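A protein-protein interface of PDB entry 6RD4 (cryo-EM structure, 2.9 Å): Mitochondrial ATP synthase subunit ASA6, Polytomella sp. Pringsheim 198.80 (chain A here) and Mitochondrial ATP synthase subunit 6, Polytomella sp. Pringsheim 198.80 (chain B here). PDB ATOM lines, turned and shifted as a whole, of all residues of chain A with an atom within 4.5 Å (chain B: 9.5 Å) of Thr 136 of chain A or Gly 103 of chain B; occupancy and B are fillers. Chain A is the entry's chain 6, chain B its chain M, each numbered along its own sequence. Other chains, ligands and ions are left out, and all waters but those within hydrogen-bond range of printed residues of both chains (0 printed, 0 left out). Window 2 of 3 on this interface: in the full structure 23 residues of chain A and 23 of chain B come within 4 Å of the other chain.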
ATOM      1  N   ARG A 130      -7.428  -1.251  25.891  1.00  0.00           N
ATOM      2  CA  ARG A 130      -7.326   0.139  25.478  1.00  0.00           C
ATOM      3  C   ARG A 130      -7.816   1.095  26.539  1.00  0.00           C
ATOM      4  O   ARG A 130      -7.438   2.261  26.511  1.00  0.00           O
ATOM      5  CB  ARG A 130      -8.120   0.374  24.212  1.00  0.00           C
ATOM      6  CG  ARG A 130      -7.381   0.032  22.993  1.00  0.00           C
ATOM      7  CD  ARG A 130      -8.143   0.424  21.782  1.00  0.00           C
ATOM      8  NE  ARG A 130      -8.083   1.847  21.540  1.00  0.00           N
ATOM      9  CZ  ARG A 130      -7.205   2.419  20.739  1.00  0.00           C
ATOM     10  NH1 ARG A 130      -6.313   1.694  20.118  1.00  0.00           N
ATOM     11  NH2 ARG A 130      -7.213   3.720  20.571  1.00  0.00           N
ATOM     12  N   GLY A 131      -8.664   0.652  27.443  1.00  0.00           N
ATOM     13  CA  GLY A 131      -9.073   1.466  28.559  1.00  0.00           C
ATOM     14  C   GLY A 131      -8.183   1.390  29.761  1.00  0.00           C
ATOM     15  O   GLY A 131      -8.342   2.188  30.677  1.00  0.00           O
ATOM     16  N   ALA A 133      -4.960   1.886  29.627  1.00  0.00           N
ATOM     17  CA  ALA A 133      -4.027   2.947  29.340  1.00  0.00           C
ATOM     18  C   ALA A 133      -4.771   4.249  29.192  1.00  0.00           C
ATOM     19  O   ALA A 133      -5.683   4.328  28.377  1.00  0.00           O
ATOM     20  CB  ALA A 133      -3.286   2.659  28.063  1.00  0.00           C
ATOM     21  N   PRO A 134      -4.412   5.295  29.931  1.00  0.00           N
ATOM     22  CA  PRO A 134      -5.056   6.591  29.721  1.00  0.00           C
ATOM     23  C   PRO A 134      -4.740   7.229  28.390  1.00  0.00           C
ATOM     24  O   PRO A 134      -5.457   8.145  27.994  1.00  0.00           O
ATOM     25  CB  PRO A 134      -4.508   7.432  30.870  1.00  0.00           C
ATOM     26  CG  PRO A 134      -4.049   6.497  31.826  1.00  0.00           C
ATOM     27  CD  PRO A 134      -3.529   5.338  31.092  1.00  0.00           C
ATOM     28  N   ALA A 135      -3.704   6.775  27.689  1.00  0.00           N
ATOM     29  CA  ALA A 135      -3.373   7.304  26.378  1.00  0.00           C
ATOM     30  C   ALA A 135      -4.367   6.878  25.319  1.00  0.00           C
ATOM     31  O   ALA A 135      -4.519   7.562  24.308  1.00  0.00           O
ATOM     32  CB  ALA A 135      -1.988   6.845  25.976  1.00  0.00           C
ATOM     33  N   THR A 136      -5.024   5.749  25.501  1.00  0.00           N
ATOM     34  CA  THR A 136      -5.976   5.251  24.530  1.00  0.00           C
ATOM     35  C   THR A 136      -7.393   5.248  25.063  1.00  0.00           C
ATOM     36  O   THR A 136      -8.322   4.962  24.317  1.00  0.00           O
ATOM     37  CB  THR A 136      -5.599   3.843  24.106  1.00  0.00           C
ATOM     38  OG1 THR A 136      -5.565   3.022  25.261  1.00  0.00           O
ATOM     39  CG2 THR A 136      -4.259   3.809  23.503  1.00  0.00           C
ATOM     40  N   ALA A 137      -7.579   5.550  26.334  1.00  0.00           N
ATOM     41  CA  ALA A 137      -8.897   5.633  26.921  1.00  0.00           C
ATOM     42  C   ALA A 137      -9.638   6.902  26.538  1.00  0.00           C
ATOM     43  O   ALA A 137     -10.837   6.997  26.804  1.00  0.00           O
ATOM     44  CB  ALA A 137      -8.786   5.544  28.435  1.00  0.00           C
ATOM     45  N   SER A 138      -8.969   7.872  25.926  1.00  0.00           N
ATOM     46  CA  SER A 138      -9.579   9.133  25.547  1.00  0.00           C
ATOM     47  C   SER A 138      -9.035   9.520  24.187  1.00  0.00           C
ATOM     48  O   SER A 138      -8.339   8.746  23.532  1.00  0.00           O
ATOM     49  CB  SER A 138      -9.282  10.211  26.586  1.00  0.00           C
ATOM     50  OG  SER A 138      -9.796   9.859  27.844  1.00  0.00           O
ATOM     51  N   VAL B 100       8.067   1.461  17.637  1.00  0.00           N
ATOM     52  CA  VAL B 100       6.915   0.991  18.372  1.00  0.00           C
ATOM     53  C   VAL B 100       5.708   1.714  17.825  1.00  0.00           C
ATOM     54  O   VAL B 100       5.755   2.925  17.622  1.00  0.00           O
ATOM     55  CB  VAL B 100       7.068   1.258  19.873  1.00  0.00           C
ATOM     56  CG1 VAL B 100       5.978   0.584  20.616  1.00  0.00           C
ATOM     57  CG2 VAL B 100       8.386   0.799  20.344  1.00  0.00           C
ATOM     58  N   LYS B 101       4.650   0.983  17.559  1.00  0.00           N
ATOM     59  CA  LYS B 101       3.386   1.620  17.269  1.00  0.00           C
ATOM     60  C   LYS B 101       2.795   2.150  18.552  1.00  0.00           C
ATOM     61  O   LYS B 101       2.862   1.492  19.588  1.00  0.00           O
ATOM     62  CB  LYS B 101       2.452   0.612  16.645  1.00  0.00           C
ATOM     63  CG  LYS B 101       1.119   1.125  16.304  1.00  0.00           C
ATOM     64  CD  LYS B 101       0.471   0.171  15.396  1.00  0.00           C
ATOM     65  CE  LYS B 101       0.074  -1.036  16.116  1.00  0.00           C
ATOM     66  NZ  LYS B 101      -1.190  -0.754  16.774  1.00  0.00           N
ATOM     67  N   THR B 102       2.234   3.351  18.509  1.00  0.00           N
ATOM     68  CA  THR B 102       1.577   3.860  19.696  1.00  0.00           C
ATOM     69  C   THR B 102       0.263   3.139  19.867  1.00  0.00           C
ATOM     70  O   THR B 102      -0.384   2.778  18.892  1.00  0.00           O
ATOM     71  CB  THR B 102       1.316   5.355  19.625  1.00  0.00           C
ATOM     72  OG1 THR B 102       0.491   5.631  18.509  1.00  0.00           O
ATOM     73  CG2 THR B 102       2.579   6.122  19.501  1.00  0.00           C
ATOM     74  N   GLY B 103      -0.115   2.898  21.112  1.00  0.00           N
ATOM     75  CA  GLY B 103      -1.385   2.271  21.370  1.00  0.00           C
ATOM     76  C   GLY B 103      -1.425   0.809  21.047  1.00  0.00           C
ATOM     77  O   GLY B 103      -2.490   0.285  20.732  1.00  0.00           O
ATOM     78  N   SER B 104      -0.283   0.135  21.101  1.00  0.00           N
ATOM     79  CA  SER B 104      -0.227  -1.303  20.969  1.00  0.00           C
ATOM     80  C   SER B 104      -0.895  -1.945  22.160  1.00  0.00           C
ATOM     81  O   SER B 104      -0.986  -1.350  23.222  1.00  0.00           O
ATOM     82  CB  SER B 104       1.210  -1.760  20.913  1.00  0.00           C
ATOM     83  OG  SER B 104       1.820  -1.326  19.738  1.00  0.00           O
ATOM     84  N   LEU B 105      -1.361  -3.169  21.995  1.00  0.00           N
ATOM     85  CA  LEU B 105      -1.933  -3.882  23.133  1.00  0.00           C
ATOM     86  C   LEU B 105      -0.933  -4.250  24.231  1.00  0.00           C
ATOM     87  O   LEU B 105      -1.338  -4.212  25.403  1.00  0.00           O
ATOM     88  CB  LEU B 105      -2.696  -5.107  22.627  1.00  0.00           C
ATOM     89  CG  LEU B 105      -3.424  -6.026  23.586  1.00  0.00           C
ATOM     90  CD1 LEU B 105      -4.679  -6.472  22.977  1.00  0.00           C
ATOM     91  CD2 LEU B 105      -2.600  -7.241  23.832  1.00  0.00           C
ATOM     92  N   PRO B 106       0.325  -4.635  23.970  1.00  0.00           N
ATOM     93  CA  PRO B 106       1.240  -4.806  25.102  1.00  0.00           C
ATOM     94  C   PRO B 106       1.646  -3.516  25.773  1.00  0.00           C
ATOM     95  O   PRO B 106       2.037  -3.540  26.938  1.00  0.00           O
ATOM     96  CB  PRO B 106       2.436  -5.500  24.464  1.00  0.00           C
ATOM     97  CG  PRO B 106       1.896  -6.168  23.365  1.00  0.00           C
ATOM     98  CD  PRO B 106       0.922  -5.270  22.786  1.00  0.00           C
ATOM     99  N   THR B 107       1.588  -2.397  25.071  1.00  0.00           N
ATOM    100  CA  THR B 107       1.859  -1.102  25.671  1.00  0.00           C
ATOM    101  C   THR B 107       0.698  -0.660  26.535  1.00  0.00           C
ATOM    102  O   THR B 107       0.891  -0.011  27.558  1.00  0.00           O
ATOM    103  CB  THR B 107       2.126  -0.099  24.559  1.00  0.00           C
ATOM    104  OG1 THR B 107       3.145  -0.617  23.708  1.00  0.00           O
ATOM    105  CG2 THR B 107       2.579   1.217  25.074  1.00  0.00           C
ATOM    106  N   ASN B 108      -0.519  -1.025  26.148  1.00  0.00           N
ATOM    107  CA  ASN B 108      -1.695  -0.661  26.920  1.00  0.00           C
ATOM    108  C   ASN B 108      -1.867  -1.553  28.129  1.00  0.00           C
ATOM    109  O   ASN B 108      -2.382  -1.119  29.153  1.00  0.00           O
ATOM    110  CB  ASN B 108      -2.932  -0.753  26.054  1.00  0.00           C
ATOM    111  CG  ASN B 108      -2.936   0.220  24.962  1.00  0.00           C
ATOM    112  OD1 ASN B 108      -3.561   0.002  23.943  1.00  0.00           O
ATOM    113  ND2 ASN B 108      -2.219   1.302  25.138  1.00  0.00           N
ATOM    114  N   PHE B 109      -1.504  -2.821  28.007  1.00  0.00           N
ATOM    115  CA  PHE B 109      -1.586  -3.717  29.145  1.00  0.00           C
ATOM    116  C   PHE B 109      -0.550  -3.356  30.190  1.00  0.00           C
ATOM    117  O   PHE B 109      -0.886  -3.161  31.355  1.00  0.00           O
ATOM    118  CB  PHE B 109      -1.416  -5.152  28.682  1.00  0.00           C
ATOM    119  CG  PHE B 109      -1.469  -6.149  29.783  1.00  0.00           C
ATOM    120  CD1 PHE B 109      -2.638  -6.378  30.463  1.00  0.00           C
ATOM    121  CD2 PHE B 109      -0.357  -6.882  30.119  1.00  0.00           C
ATOM    122  CE1 PHE B 109      -2.689  -7.293  31.462  1.00  0.00           C
ATOM    123  CE2 PHE B 109      -0.407  -7.793  31.123  1.00  0.00           C
ATOM    124  CZ  PHE B 109      -1.574  -7.995  31.792  1.00  0.00           C
ATOM    125  N   THR B 111       0.907  -0.530  30.611  1.00  0.00           N
ATOM    126  CA  THR B 111       0.606   0.758  31.219  1.00  0.00           C
ATOM    127  C   THR B 111      -0.367   0.588  32.357  1.00  0.00           C
ATOM    128  O   THR B 111      -0.184   1.150  33.430  1.00  0.00           O
ATOM    129  CB  THR B 111       0.007   1.703  30.201  1.00  0.00           C
ATOM    130  OG1 THR B 111       0.856   1.763  29.066  1.00  0.00           O
ATOM    131  CG2 THR B 111      -0.124   3.055  30.776  1.00  0.00           C
ATOM    132  N   GLY B 112      -1.406  -0.201  32.143  1.00  0.00           N
ATOM    133  CA  GLY B 112      -2.370  -0.418  33.190  1.00  0.00           C
ATOM    134  C   GLY B 112      -1.844  -1.271  34.311  1.00  0.00           C
ATOM    135  O   GLY B 112      -2.283  -1.132  35.445  1.00  0.00           O
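Of chain B, only Gly 103 (3.9 Å) and Asn 108 (3.6 Å) come within 4 Å of Thr 136 of chain A.
Of chain A, only Thr 136 comes within 4 Å of Gly 103 of chain B.
Ala 133 of chain A touches just one residue of chain B: Asn 108.
No residue of chain B comes within 4 Å of Ala 135 of chain A.
Printed residues of chain A within 4 Å of Asn 108 of chain B: Arg 130, Ala 133 and Thr 136.
The nearest residue of chain B that does not touch Thr 136 of chain A is Thr 102 of chain B (5.8 Å).
The side-chain amide oxygen of Asn 108 of chain B sits close to the backbone carbonyl oxygen of Gly 103 of chain B, at 3.4 Å.
The side-chain amide oxygen (OD1) of Asn 108 of chain B sits close to the backbone carbonyl oxygen (O) of Ser 104 of chain B (3.0 Å).
N of Ala 137 of chain A lies within hydrogen-bond range of O of Arg 130 of chain A (3.3 Å).
The backbone carbonyl oxygen (O) of Ala 133 of chain A sits at hydrogen-bond distance from the side-chain hydroxyl (OG1) of Thr 136 of chain A, 3.4 Å away.
Asn 108 of chain B touches Arg 130 of chain A.
Ala 133 of chain A touches Asn 108 of chain B (CB to ND2, 3.4 Å).
Gly 103 of chain B touches Thr 136 of chain A (CA to CG2, 3.9 Å).
CG2 of Thr 136 of chain A touches ND2 of Asn 108 of chain B, at 3.6 Å.
Printed residues of chain B that touch a printed residue of chain A: Gly 103 and Asn 108.
Among the printed residues, 4 pairs touch across the chains.
Among the printed residues, no Asp or Glu carboxylate lies within 4 Å of a Lys or Arg side-chain nitrogen of the other chain.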
